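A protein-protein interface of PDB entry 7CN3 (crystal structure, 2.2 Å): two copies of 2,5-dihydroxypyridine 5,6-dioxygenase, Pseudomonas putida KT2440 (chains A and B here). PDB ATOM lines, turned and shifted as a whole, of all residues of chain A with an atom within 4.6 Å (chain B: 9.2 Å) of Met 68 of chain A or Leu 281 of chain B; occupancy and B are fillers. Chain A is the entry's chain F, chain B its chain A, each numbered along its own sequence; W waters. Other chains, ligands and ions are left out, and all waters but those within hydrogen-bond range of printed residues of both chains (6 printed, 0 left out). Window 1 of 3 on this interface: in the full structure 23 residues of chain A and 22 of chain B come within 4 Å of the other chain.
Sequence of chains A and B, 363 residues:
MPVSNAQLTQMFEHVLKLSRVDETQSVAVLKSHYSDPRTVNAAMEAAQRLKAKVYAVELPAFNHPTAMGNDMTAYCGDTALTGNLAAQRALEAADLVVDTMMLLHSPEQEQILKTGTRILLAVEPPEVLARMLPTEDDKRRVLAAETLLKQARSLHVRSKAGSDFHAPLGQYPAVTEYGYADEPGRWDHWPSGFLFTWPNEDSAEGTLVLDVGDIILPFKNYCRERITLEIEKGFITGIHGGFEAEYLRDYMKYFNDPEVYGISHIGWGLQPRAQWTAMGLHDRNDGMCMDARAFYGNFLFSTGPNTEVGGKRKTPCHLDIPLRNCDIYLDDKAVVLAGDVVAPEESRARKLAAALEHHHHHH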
ATOM      1  N   THR A  66     -20.213 -27.998  29.015  1.00  0.00           N
ATOM      2  CA  THR A  66     -19.170 -27.877  28.001  1.00  0.00           C
ATOM      3  C   THR A  66     -19.709 -27.789  26.580  1.00  0.00           C
ATOM      4  O   THR A  66     -18.922 -27.573  25.655  1.00  0.00           O
ATOM      5  CB  THR A  66     -18.193 -29.060  28.085  1.00  0.00           C
ATOM      6  OG1 THR A  66     -18.870 -30.271  27.734  1.00  0.00           O
ATOM      7  CG2 THR A  66     -17.583 -29.200  29.531  1.00  0.00           C
ATOM      8  N   ALA A  67     -21.013 -27.950  26.371  1.00  0.00           N
ATOM      9  CA  ALA A  67     -21.560 -27.830  25.028  1.00  0.00           C
ATOM     10  C   ALA A  67     -21.444 -26.393  24.521  1.00  0.00           C
ATOM     11  O   ALA A  67     -21.670 -25.426  25.258  1.00  0.00           O
ATOM     12  CB  ALA A  67     -23.021 -28.295  25.005  1.00  0.00           C
ATOM     13  N   MET A  68     -21.080 -26.257  23.255  1.00  0.00           N
ATOM     14  CA  MET A  68     -20.996 -24.968  22.587  1.00  0.00           C
ATOM     15  C   MET A  68     -22.094 -24.827  21.535  1.00  0.00           C
ATOM     16  O   MET A  68     -22.568 -25.815  20.970  1.00  0.00           O
ATOM     17  CB  MET A  68     -19.622 -24.784  21.935  1.00  0.00           C
ATOM     18  CG  MET A  68     -18.461 -24.898  22.912  1.00  0.00           C
ATOM     19  SD  MET A  68     -16.917 -24.500  22.096  1.00  0.00           S
ATOM     20  CE  MET A  68     -16.585 -26.030  21.243  1.00  0.00           C
ATOM     21  N   GLY A  69     -22.493 -23.584  21.268  1.00  0.00           N
ATOM     22  CA  GLY A  69     -23.504 -23.314  20.262  1.00  0.00           C
ATOM     23  C   GLY A  69     -24.904 -23.716  20.686  1.00  0.00           C
ATOM     24  O   GLY A  69     -25.084 -24.309  21.748  1.00  0.00           O
ATOM     25  N   ASN A  70     -25.902 -23.414  19.853  1.00  0.00           N
ATOM     26  CA  ASN A  70     -27.304 -23.643  20.183  1.00  0.00           C
ATOM     27  C   ASN A  70     -27.923 -24.823  19.453  1.00  0.00           C
ATOM     28  O   ASN A  70     -29.133 -25.041  19.587  1.00  0.00           O
ATOM     29  CB  ASN A  70     -28.144 -22.394  19.872  1.00  0.00           C
ATOM     30  CG  ASN A  70     -27.731 -21.194  20.697  1.00  0.00           C
ATOM     31  OD1 ASN A  70     -27.492 -20.106  20.163  1.00  0.00           O
ATOM     32  ND2 ASN A  70     -27.628 -21.392  22.008  1.00  0.00           N
ATOM     33  N   ALA A  74     -25.586 -31.097  18.880  1.00  0.00           N
ATOM     34  CA  ALA A  74     -24.150 -30.934  19.049  1.00  0.00           C
ATOM     35  C   ALA A  74     -23.618 -31.782  20.197  1.00  0.00           C
ATOM     36  O   ALA A  74     -22.546 -32.381  20.062  1.00  0.00           O
ATOM     37  CB  ALA A  74     -23.802 -29.457  19.256  1.00  0.00           C
ATOM     38  N   PRO A 218     -22.631 -29.986  13.222  1.00  0.00           N
ATOM     39  CA  PRO A 218     -23.396 -28.740  13.244  1.00  0.00           C
ATOM     40  C   PRO A 218     -22.643 -27.471  12.861  1.00  0.00           C
ATOM     41  O   PRO A 218     -23.182 -26.399  13.154  1.00  0.00           O
ATOM     42  CB  PRO A 218     -23.822 -28.661  14.705  1.00  0.00           C
ATOM     43  CG  PRO A 218     -22.615 -29.208  15.437  1.00  0.00           C
ATOM     44  CD  PRO A 218     -22.025 -30.275  14.538  1.00  0.00           C
ATOM     45  N   PHE A 219     -21.457 -27.553  12.233  1.00  0.00           N
ATOM     46  CA  PHE A 219     -20.756 -26.319  11.862  1.00  0.00           C
ATOM     47  C   PHE A 219     -21.583 -25.502  10.879  1.00  0.00           C
ATOM     48  O   PHE A 219     -21.550 -24.270  10.903  1.00  0.00           O
ATOM     49  CB  PHE A 219     -19.381 -26.600  11.239  1.00  0.00           C
ATOM     50  CG  PHE A 219     -18.459 -27.426  12.091  1.00  0.00           C
ATOM     51  CD1 PHE A 219     -18.729 -27.673  13.427  1.00  0.00           C
ATOM     52  CD2 PHE A 219     -17.294 -27.948  11.533  1.00  0.00           C
ATOM     53  CE1 PHE A 219     -17.864 -28.448  14.192  1.00  0.00           C
ATOM     54  CE2 PHE A 219     -16.414 -28.721  12.290  1.00  0.00           C
ATOM     55  CZ  PHE A 219     -16.698 -28.970  13.614  1.00  0.00           C
ATOM     56  N   TYR A 247      -9.806 -26.548  12.032  1.00  0.00           N
ATOM     57  CA  TYR A 247     -10.959 -26.256  12.865  1.00  0.00           C
ATOM     58  C   TYR A 247     -11.594 -27.547  13.353  1.00  0.00           C
ATOM     59  O   TYR A 247     -11.849 -27.718  14.551  1.00  0.00           O
ATOM     60  CB  TYR A 247     -11.966 -25.404  12.073  1.00  0.00           C
ATOM     61  CG  TYR A 247     -13.182 -24.993  12.864  1.00  0.00           C
ATOM     62  CD1 TYR A 247     -14.256 -25.858  13.022  1.00  0.00           C
ATOM     63  CD2 TYR A 247     -13.256 -23.743  13.462  1.00  0.00           C
ATOM     64  CE1 TYR A 247     -15.365 -25.486  13.748  1.00  0.00           C
ATOM     65  CE2 TYR A 247     -14.378 -23.356  14.196  1.00  0.00           C
ATOM     66  CZ  TYR A 247     -15.421 -24.233  14.329  1.00  0.00           C
ATOM     67  OH  TYR A 247     -16.524 -23.869  15.061  1.00  0.00           O
ATOM     68  N   TYR A 251     -11.900 -28.924  17.070  1.00  0.00           N
ATOM     69  CA  TYR A 251     -13.206 -29.156  17.682  1.00  0.00           C
ATOM     70  C   TYR A 251     -13.305 -30.565  18.269  1.00  0.00           C
ATOM     71  O   TYR A 251     -13.789 -30.740  19.393  1.00  0.00           O
ATOM     72  CB  TYR A 251     -14.322 -28.908  16.662  1.00  0.00           C
ATOM     73  CG  TYR A 251     -15.732 -29.092  17.210  1.00  0.00           C
ATOM     74  CD1 TYR A 251     -16.366 -28.075  17.929  1.00  0.00           C
ATOM     75  CD2 TYR A 251     -16.426 -30.281  17.014  1.00  0.00           C
ATOM     76  CE1 TYR A 251     -17.652 -28.241  18.433  1.00  0.00           C
ATOM     77  CE2 TYR A 251     -17.715 -30.459  17.517  1.00  0.00           C
ATOM     78  CZ  TYR A 251     -18.320 -29.434  18.223  1.00  0.00           C
ATOM     79  OH  TYR A 251     -19.596 -29.603  18.713  1.00  0.00           O
ATOM     80  N   TYR A 254     -11.283 -31.160  21.567  1.00  0.00           N
ATOM     81  CA  TYR A 254     -11.754 -30.485  22.775  1.00  0.00           C
ATOM     82  C   TYR A 254     -12.558 -31.406  23.679  1.00  0.00           C
ATOM     83  O   TYR A 254     -12.554 -31.229  24.903  1.00  0.00           O
ATOM     84  CB  TYR A 254     -12.575 -29.264  22.358  1.00  0.00           C
ATOM     85  CG  TYR A 254     -13.606 -28.721  23.328  1.00  0.00           C
ATOM     86  CD1 TYR A 254     -13.227 -27.945  24.420  1.00  0.00           C
ATOM     87  CD2 TYR A 254     -14.966 -28.920  23.102  1.00  0.00           C
ATOM     88  CE1 TYR A 254     -14.166 -27.412  25.267  1.00  0.00           C
ATOM     89  CE2 TYR A 254     -15.911 -28.399  23.942  1.00  0.00           C
ATOM     90  CZ  TYR A 254     -15.509 -27.640  25.027  1.00  0.00           C
ATOM     91  OH  TYR A 254     -16.451 -27.102  25.876  1.00  0.00           O
ATOM     92  N   ARG A 284     -27.577 -19.899  11.758  1.00  0.00           N
ATOM     93  CA  ARG A 284     -27.259 -21.143  12.447  1.00  0.00           C
ATOM     94  C   ARG A 284     -28.310 -21.503  13.487  1.00  0.00           C
ATOM     95  O   ARG A 284     -28.563 -22.694  13.727  1.00  0.00           O
ATOM     96  CB  ARG A 284     -25.900 -21.041  13.126  1.00  0.00           C
ATOM     97  CG  ARG A 284     -24.760 -20.636  12.225  1.00  0.00           C
ATOM     98  CD  ARG A 284     -23.458 -20.939  12.947  1.00  0.00           C
ATOM     99  NE  ARG A 284     -22.373 -21.205  12.013  1.00  0.00           N
ATOM    100  CZ  ARG A 284     -21.575 -20.267  11.528  1.00  0.00           C
ATOM    101  NH1 ARG A 284     -21.738 -19.007  11.903  1.00  0.00           N
ATOM    102  NH2 ARG A 284     -20.611 -20.598  10.679  1.00  0.00           N
ATOM    103  N   PRO B   2     -29.603 -26.163  26.796  1.00  0.00           N
ATOM    104  CA  PRO B   2     -30.039 -24.808  27.157  1.00  0.00           C
ATOM    105  C   PRO B   2     -30.198 -24.660  28.664  1.00  0.00           C
ATOM    106  O   PRO B   2     -30.353 -25.687  29.349  1.00  0.00           O
ATOM    107  CB  PRO B   2     -31.384 -24.660  26.445  1.00  0.00           C
ATOM    108  CG  PRO B   2     -31.316 -25.625  25.301  1.00  0.00           C
ATOM    109  CD  PRO B   2     -30.461 -26.770  25.766  1.00  0.00           C
ATOM    110  N   GLU B 127     -26.304 -19.856  28.008  1.00  0.00           N
ATOM    111  CA  GLU B 127     -25.473 -21.045  27.861  1.00  0.00           C
ATOM    112  C   GLU B 127     -23.994 -20.682  27.887  1.00  0.00           C
ATOM    113  O   GLU B 127     -23.165 -21.446  28.397  1.00  0.00           O
ATOM    114  CB  GLU B 127     -25.832 -21.793  26.572  1.00  0.00           C
ATOM    115  CG  GLU B 127     -27.249 -22.404  26.590  1.00  0.00           C
ATOM    116  CD  GLU B 127     -28.345 -21.341  26.555  1.00  0.00           C
ATOM    117  OE1 GLU B 127     -28.097 -20.248  25.980  1.00  0.00           O
ATOM    118  OE2 GLU B 127     -29.440 -21.593  27.111  1.00  0.00           O
ATOM    119  N   VAL B 128     -23.647 -19.523  27.336  1.00  0.00           N
ATOM    120  CA  VAL B 128     -22.267 -19.067  27.381  1.00  0.00           C
ATOM    121  C   VAL B 128     -21.881 -18.703  28.815  1.00  0.00           C
ATOM    122  O   VAL B 128     -20.778 -19.021  29.272  1.00  0.00           O
ATOM    123  CB  VAL B 128     -22.080 -17.886  26.407  1.00  0.00           C
ATOM    124  CG1 VAL B 128     -20.673 -17.331  26.511  1.00  0.00           C
ATOM    125  CG2 VAL B 128     -22.415 -18.310  24.951  1.00  0.00           C
ATOM    126  N   ARG B 131     -21.131 -22.043  30.504  1.00  0.00           N
ATOM    127  CA  ARG B 131     -19.896 -22.711  30.110  1.00  0.00           C
ATOM    128  C   ARG B 131     -18.686 -22.085  30.795  1.00  0.00           C
ATOM    129  O   ARG B 131     -17.716 -22.787  31.122  1.00  0.00           O
ATOM    130  CB  ARG B 131     -19.732 -22.652  28.586  1.00  0.00           C
ATOM    131  CG  ARG B 131     -18.534 -23.448  28.064  1.00  0.00           C
ATOM    132  CD  ARG B 131     -18.760 -23.954  26.634  1.00  0.00           C
ATOM    133  NE  ARG B 131     -19.262 -22.927  25.736  1.00  0.00           N
ATOM    134  CZ  ARG B 131     -18.549 -21.886  25.325  1.00  0.00           C
ATOM    135  NH1 ARG B 131     -17.295 -21.730  25.743  1.00  0.00           N
ATOM    136  NH2 ARG B 131     -19.090 -20.999  24.507  1.00  0.00           N
ATOM    137  N   MET B 132     -18.725 -20.777  31.040  1.00  0.00           N
ATOM    138  CA  MET B 132     -17.589 -20.094  31.639  1.00  0.00           C
ATOM    139  C   MET B 132     -17.983 -19.486  32.979  1.00  0.00           C
ATOM    140  O   MET B 132     -17.633 -18.344  33.286  1.00  0.00           O
ATOM    141  CB  MET B 132     -17.020 -19.045  30.684  1.00  0.00           C
ATOM    142  CG  MET B 132     -16.318 -19.636  29.473  1.00  0.00           C
ATOM    143  SD  MET B 132     -15.777 -18.391  28.278  1.00  0.00           S
ATOM    144  CE  MET B 132     -17.284 -18.094  27.327  1.00  0.00           C
ATOM    145  N   LYS B 220     -16.358 -10.978  13.233  1.00  0.00           N
ATOM    146  CA  LYS B 220     -16.695 -12.338  13.653  1.00  0.00           C
ATOM    147  C   LYS B 220     -16.526 -13.360  12.521  1.00  0.00           C
ATOM    148  O   LYS B 220     -17.383 -14.219  12.299  1.00  0.00           O
ATOM    149  CB  LYS B 220     -18.114 -12.394  14.245  1.00  0.00           C
ATOM    150  CG  LYS B 220     -18.254 -11.786  15.674  1.00  0.00           C
ATOM    151  CD  LYS B 220     -19.705 -11.426  15.982  1.00  0.00           C
ATOM    152  CE  LYS B 220     -19.836 -10.624  17.263  1.00  0.00           C
ATOM    153  NZ  LYS B 220     -21.074  -9.775  17.284  1.00  0.00           N
ATOM    154  N   TYR B 222     -13.443 -16.078  10.730  1.00  0.00           N
ATOM    155  CA  TYR B 222     -12.101 -16.656  10.682  1.00  0.00           C
ATOM    156  C   TYR B 222     -11.452 -16.236   9.358  1.00  0.00           C
ATOM    157  O   TYR B 222     -12.009 -16.505   8.286  1.00  0.00           O
ATOM    158  CB  TYR B 222     -12.155 -18.183  10.786  1.00  0.00           C
ATOM    159  CG  TYR B 222     -12.785 -18.734  12.064  1.00  0.00           C
ATOM    160  CD1 TYR B 222     -12.025 -18.903  13.216  1.00  0.00           C
ATOM    161  CD2 TYR B 222     -14.128 -19.067  12.117  1.00  0.00           C
ATOM    162  CE1 TYR B 222     -12.583 -19.398  14.385  1.00  0.00           C
ATOM    163  CE2 TYR B 222     -14.707 -19.575  13.288  1.00  0.00           C
ATOM    164  CZ  TYR B 222     -13.924 -19.737  14.419  1.00  0.00           C
ATOM    165  OH  TYR B 222     -14.461 -20.222  15.591  1.00  0.00           O
ATOM    166  N   PRO B 272      -9.250 -21.343  29.820  1.00  0.00           N
ATOM    167  CA  PRO B 272      -9.268 -22.624  29.102  1.00  0.00           C
ATOM    168  C   PRO B 272     -10.670 -23.105  28.755  1.00  0.00           C
ATOM    169  O   PRO B 272     -10.809 -23.959  27.868  1.00  0.00           O
ATOM    170  CB  PRO B 272      -8.561 -23.583  30.076  1.00  0.00           C
ATOM    171  CG  PRO B 272      -8.862 -23.012  31.435  1.00  0.00           C
ATOM    172  CD  PRO B 272      -8.908 -21.501  31.247  1.00  0.00           C
ATOM    173  N   ARG B 273     -11.714 -22.573  29.389  1.00  0.00           N
ATOM    174  CA  ARG B 273     -13.075 -22.974  29.042  1.00  0.00           C
ATOM    175  C   ARG B 273     -13.680 -22.131  27.916  1.00  0.00           C
ATOM    176  O   ARG B 273     -14.763 -22.471  27.413  1.00  0.00           O
ATOM    177  CB  ARG B 273     -13.969 -22.939  30.291  1.00  0.00           C
ATOM    178  CG  ARG B 273     -13.577 -23.980  31.368  1.00  0.00           C
ATOM    179  CD  ARG B 273     -14.436 -23.864  32.634  1.00  0.00           C
ATOM    180  NE  ARG B 273     -14.112 -22.663  33.414  1.00  0.00           N
ATOM    181  CZ  ARG B 273     -14.999 -21.969  34.123  1.00  0.00           C
ATOM    182  NH1 ARG B 273     -16.274 -22.355  34.152  1.00  0.00           N
ATOM    183  NH2 ARG B 273     -14.617 -20.885  34.793  1.00  0.00           N
ATOM    184  N   ALA B 274     -13.012 -21.052  27.509  1.00  0.00           N
ATOM    185  CA  ALA B 274     -13.332 -20.386  26.253  1.00  0.00           C
ATOM    186  C   ALA B 274     -12.659 -21.133  25.109  1.00  0.00           C
ATOM    187  O   ALA B 274     -11.625 -21.781  25.297  1.00  0.00           O
ATOM    188  CB  ALA B 274     -12.863 -18.928  26.258  1.00  0.00           C
ATOM    189  N   GLN B 275     -13.243 -21.032  23.913  1.00  0.00           N
ATOM    190  CA  GLN B 275     -12.797 -21.859  22.801  1.00  0.00           C
ATOM    191  C   GLN B 275     -12.743 -21.056  21.512  1.00  0.00           C
ATOM    192  O   GLN B 275     -13.722 -20.398  21.134  1.00  0.00           O
ATOM    193  CB  GLN B 275     -13.698 -23.084  22.632  1.00  0.00           C
ATOM    194  CG  GLN B 275     -13.542 -24.092  23.762  1.00  0.00           C
ATOM    195  CD  GLN B 275     -12.196 -24.800  23.754  1.00  0.00           C
ATOM    196  OE1 GLN B 275     -11.735 -25.272  22.714  1.00  0.00           O
ATOM    197  NE2 GLN B 275     -11.575 -24.902  24.919  1.00  0.00           N
ATOM    198  N   TRP B 276     -11.569 -21.104  20.870  1.00  0.00           N
ATOM    199  CA  TRP B 276     -11.371 -20.485  19.567  1.00  0.00           C
ATOM    200  C   TRP B 276     -12.397 -20.966  18.542  1.00  0.00           C
ATOM    201  O   TRP B 276     -12.797 -20.197  17.662  1.00  0.00           O
ATOM    202  CB  TRP B 276      -9.941 -20.781  19.094  1.00  0.00           C
ATOM    203  CG  TRP B 276      -9.685 -20.491  17.648  1.00  0.00           C
ATOM    204  CD1 TRP B 276      -9.521 -19.260  17.067  1.00  0.00           C
ATOM    205  CD2 TRP B 276      -9.554 -21.448  16.596  1.00  0.00           C
ATOM    206  NE1 TRP B 276      -9.295 -19.399  15.716  1.00  0.00           N
ATOM    207  CE2 TRP B 276      -9.314 -20.732  15.401  1.00  0.00           C
ATOM    208  CE3 TRP B 276      -9.602 -22.846  16.548  1.00  0.00           C
ATOM    209  CZ2 TRP B 276      -9.132 -21.363  14.179  1.00  0.00           C
ATOM    210  CZ3 TRP B 276      -9.416 -23.470  15.334  1.00  0.00           C
ATOM    211  CH2 TRP B 276      -9.184 -22.728  14.164  1.00  0.00           C
ATOM    212  N   THR B 277     -12.848 -22.224  18.652  1.00  0.00           N
ATOM    213  CA  THR B 277     -13.854 -22.749  17.735  1.00  0.00           C
ATOM    214  C   THR B 277     -15.269 -22.263  18.029  1.00  0.00           C
ATOM    215  O   THR B 277     -16.154 -22.460  17.187  1.00  0.00           O
ATOM    216  CB  THR B 277     -13.860 -24.282  17.753  1.00  0.00           C
ATOM    217  OG1 THR B 277     -14.063 -24.740  19.093  1.00  0.00           O
ATOM    218  CG2 THR B 277     -12.540 -24.841  17.205  1.00  0.00           C
ATOM    219  N   ALA B 278     -15.523 -21.639  19.184  1.00  0.00           N
ATOM    220  CA  ALA B 278     -16.913 -21.373  19.557  1.00  0.00           C
ATOM    221  C   ALA B 278     -17.581 -20.402  18.590  1.00  0.00           C
ATOM    222  O   ALA B 278     -18.764 -20.560  18.262  1.00  0.00           O
ATOM    223  CB  ALA B 278     -16.998 -20.844  20.992  1.00  0.00           C
ATOM    224  N   MET B 279     -16.841 -19.394  18.121  1.00  0.00           N
ATOM    225  CA  MET B 279     -17.450 -18.361  17.291  1.00  0.00           C
ATOM    226  C   MET B 279     -18.182 -18.961  16.098  1.00  0.00           C
ATOM    227  O   MET B 279     -19.260 -18.488  15.717  1.00  0.00           O
ATOM    228  CB  MET B 279     -16.378 -17.378  16.821  1.00  0.00           C
ATOM    229  CG  MET B 279     -16.910 -16.142  16.072  1.00  0.00           C
ATOM    230  SD  MET B 279     -15.543 -15.023  15.635  1.00  0.00           S
ATOM    231  CE  MET B 279     -14.756 -15.900  14.280  1.00  0.00           C
ATOM    232  N   GLY B 280     -17.622 -20.013  15.504  1.00  0.00           N
ATOM    233  CA  GLY B 280     -18.296 -20.607  14.359  1.00  0.00           C
ATOM    234  C   GLY B 280     -19.545 -21.395  14.685  1.00  0.00           C
ATOM    235  O   GLY B 280     -20.195 -21.900  13.768  1.00  0.00           O
ATOM    236  N   LEU B 281     -19.890 -21.538  15.958  1.00  0.00           N
ATOM    237  CA  LEU B 281     -21.118 -22.206  16.347  1.00  0.00           C
ATOM    238  C   LEU B 281     -22.238 -21.232  16.686  1.00  0.00           C
ATOM    239  O   LEU B 281     -23.314 -21.678  17.082  1.00  0.00           O
ATOM    240  CB  LEU B 281     -20.846 -23.136  17.531  1.00  0.00           C
ATOM    241  CG  LEU B 281     -19.823 -24.215  17.145  1.00  0.00           C
ATOM    242  CD1 LEU B 281     -19.283 -24.944  18.357  1.00  0.00           C
ATOM    243  CD2 LEU B 281     -20.480 -25.188  16.180  1.00  0.00           C
ATOM    244  N   HIS B 282     -22.016 -19.925  16.517  1.00  0.00           N
ATOM    245  CA  HIS B 282     -22.954 -18.876  16.904  1.00  0.00           C
ATOM    246  C   HIS B 282     -23.277 -17.966  15.722  1.00  0.00           C
ATOM    247  O   HIS B 282     -22.511 -17.862  14.764  1.00  0.00           O
ATOM    248  CB  HIS B 282     -22.382 -18.019  18.049  1.00  0.00           C
ATOM    249  CG  HIS B 282     -22.446 -18.686  19.383  1.00  0.00           C
ATOM    250  ND1 HIS B 282     -23.578 -18.662  20.170  1.00  0.00           N
ATOM    251  CD2 HIS B 282     -21.531 -19.421  20.056  1.00  0.00           C
ATOM    252  CE1 HIS B 282     -23.350 -19.340  21.281  1.00  0.00           C
ATOM    253  NE2 HIS B 282     -22.116 -19.809  21.236  1.00  0.00           N
ATOM    254  N   ASP B 283     -24.429 -17.305  15.802  1.00  0.00           N
ATOM    255  CA  ASP B 283     -24.764 -16.243  14.868  1.00  0.00           C
ATOM    256  C   ASP B 283     -24.241 -14.921  15.423  1.00  0.00           C
ATOM    257  O   ASP B 283     -23.922 -14.805  16.606  1.00  0.00           O
ATOM    258  CB  ASP B 283     -26.282 -16.159  14.630  1.00  0.00           C
ATOM    259  CG  ASP B 283     -26.842 -17.371  13.853  1.00  0.00           C
ATOM    260  OD1 ASP B 283     -26.189 -17.842  12.898  1.00  0.00           O
ATOM    261  OD2 ASP B 283     -27.957 -17.839  14.182  1.00  0.00           O
ATOM    262  N   ARG B 284     -24.155 -13.915  14.547  1.00  0.00           N
ATOM    263  CA  ARG B 284     -23.502 -12.667  14.932  1.00  0.00           C
ATOM    264  C   ARG B 284     -24.268 -11.947  16.030  1.00  0.00           C
ATOM    265  O   ARG B 284     -23.661 -11.365  16.936  1.00  0.00           O
ATOM    266  CB  ARG B 284     -23.326 -11.752  13.720  1.00  0.00           C
ATOM    267  CG  ARG B 284     -22.275 -12.243  12.743  1.00  0.00           C
ATOM    268  CD  ARG B 284     -21.971 -11.201  11.656  1.00  0.00           C
ATOM    269  NE  ARG B 284     -20.930 -11.686  10.751  1.00  0.00           N
ATOM    270  CZ  ARG B 284     -21.153 -12.190   9.538  1.00  0.00           C
ATOM    271  NH1 ARG B 284     -22.383 -12.258   9.054  1.00  0.00           N
ATOM    272  NH2 ARG B 284     -20.134 -12.619   8.808  1.00  0.00           N
ATOM    273  N   ASP B 286     -25.881 -13.104  18.478  1.00  0.00           N
ATOM    274  CA  ASP B 286     -25.980 -13.800  19.760  1.00  0.00           C
ATOM    275  C   ASP B 286     -25.294 -13.023  20.879  1.00  0.00           C
ATOM    276  O   ASP B 286     -25.692 -13.137  22.043  1.00  0.00           O
ATOM    277  CB  ASP B 286     -25.366 -15.195  19.664  1.00  0.00           C
ATOM    278  CG  ASP B 286     -26.136 -16.116  18.733  1.00  0.00           C
ATOM    279  OD1 ASP B 286     -27.172 -15.680  18.184  1.00  0.00           O
ATOM    280  OD2 ASP B 286     -25.704 -17.277  18.552  1.00  0.00           O
ATOM    281  N   CYS B 289     -19.101 -12.441  21.528  1.00  0.00           N
ATOM    282  CA  CYS B 289     -18.086 -13.500  21.420  1.00  0.00           C
ATOM    283  C   CYS B 289     -16.901 -13.218  22.350  1.00  0.00           C
ATOM    284  O   CYS B 289     -15.789 -12.873  21.932  1.00  0.00           O
ATOM    285  CB  CYS B 289     -17.600 -13.679  19.968  1.00  0.00           C
ATOM    286  SG  CYS B 289     -16.696 -15.254  19.617  1.00  0.00           S
ATOM    287  N   ASP B 291     -15.685 -15.707  23.866  1.00  0.00           N
ATOM    288  CA  ASP B 291     -14.812 -16.850  23.593  1.00  0.00           C
ATOM    289  C   ASP B 291     -13.585 -16.427  22.796  1.00  0.00           C
ATOM    290  O   ASP B 291     -12.474 -16.907  23.051  1.00  0.00           O
ATOM    291  CB  ASP B 291     -15.553 -17.923  22.807  1.00  0.00           C
ATOM    292  CG  ASP B 291     -16.298 -18.887  23.687  1.00  0.00           C
ATOM    293  OD1 ASP B 291     -15.655 -19.837  24.190  1.00  0.00           O
ATOM    294  OD2 ASP B 291     -17.533 -18.719  23.831  1.00  0.00           O
HETATM  295  O   HOH W   1     -15.480 -25.207  27.888  1.00  0.00           O
HETATM  296  O   HOH W   2     -22.057 -22.728  25.795  1.00  0.00           O
HETATM  297  O   HOH W   3     -21.315 -21.530  23.071  1.00  0.00           O
HETATM  298  O   HOH W   4     -26.456 -17.879  21.517  1.00  0.00           O
HETATM  299  O   HOH W   5     -17.991 -23.475  12.075  1.00  0.00           O
HETATM  300  O   HOH W   6     -26.409 -19.784  23.788  1.00  0.00           O
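O of Thr 277 of chain B is in hydrogen-bond range of OH of Tyr 247 of chain A (2.6 Å).
The backbone carbonyl oxygen (O) of Gly 280 of chain B is in hydrogen-bond range of the guanidinium group (NE) of Arg 284 of chain A (2.9 Å).
O of His 282 of chain B lies within hydrogen-bond range of NH1 of Arg 284 of chain A (3.2 Å).
N of Arg 284 of chain A lies within hydrogen-bond range of OD1 of Asp 283 of chain B (2.7 Å).
NH1 of Arg 131 of chain B lies within hydrogen-bond range of O of Arg 273 of chain B, 3.1 Å away.
The backbone carbonyl oxygen (O) of Phe 219 of chain A is in hydrogen-bond range of the guanidinium group (NE) of Arg 284 of chain A, at 3.4 Å.
Among the printed residues, pairs that only touch across the chains: Thr 66 of chain A with Arg 131 of chain B (3.8 Å), Ala 67 of chain A with Arg 131 of chain B (3.5 Å), Met 68 of chain A with Arg 131 of chain B (3.5 Å), Met 68 of chain A with Gln 275 of chain B (3.6 Å), Met 68 of chain A with Thr 277 of chain B (3.6 Å), Met 68 of chain A with Ala 278 of chain B (3.8 Å), Met 68 of chain A with Leu 281 of chain B (3.6 Å), Gly 69 of chain A with Leu 281 of chain B (3.6 Å), Gly 69 of chain A with His 282 of chain B (3.8 Å), Asn 70 of chain A with Asp 286 of chain B (3.7 Å), Phe 219 of chain A with Gly 280 of chain B (3.96 Å), Tyr 247 of chain A with Tyr 222 of chain B (3.4 Å), Tyr 247 of chain A with Gly 280 of chain B (3.8 Å), Tyr 247 of chain A with Leu 281 of chain B (3.9 Å), Tyr 251 of chain A with Leu 281 of chain B (3.7 Å), Tyr 254 of chain A with Arg 131 of chain B (3.98 Å), Tyr 254 of chain A with Gln 275 of chain B (3.4 Å) and Arg 284 of chain A with Leu 281 of chain B (3.9 Å).
Ala 67 of chain A touches just one residue of chain B: Arg 131 (3.5 Å).
Gly 69 of chain A touches just these residues of chain B: Leu 281 and His 282.
Of the printed residues of chain B, Tyr 251 of chain A touches Leu 281 (3.7 Å).
Printed residues of chain A within 4 Å of Tyr 222 of chain B: Tyr 247.
Of the printed residues of chain A, Gln 275 of chain B touches Met 68 (3.6 Å) and Tyr 254 (3.4 Å).
The nearest residue of chain B that does not touch Met 68 of chain A is His 282 of chain B (5.0 Å).
The nearest printed residue of chain B that does not touch Arg 284 of chain A is Met 279 of chain B (4.6 Å).
Of the 12 printed residues of chain A, 10 touch a printed residue of chain B.
Hydrophobic or aromatic side chains of chain A within 4 Å of the printed part of chain B: Met 68, Tyr 247, Tyr 251 and Tyr 254.
Among the printed residues, no Asp or Glu carboxylate lies within 4 Å of a Lys or Arg side-chain nitrogen of the other chain.
1 position is printed for both chains.
Water W3 lies within hydrogen-bond range of NE2 of His 282 of chain B, NH2 of Arg 131 of chain B and N of Gly 69 of chain A.
Water W2 lies within hydrogen-bond range of O of Ala 67 of chain A, NE of Arg 131 of chain B and O of Glu 127 of chain B.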
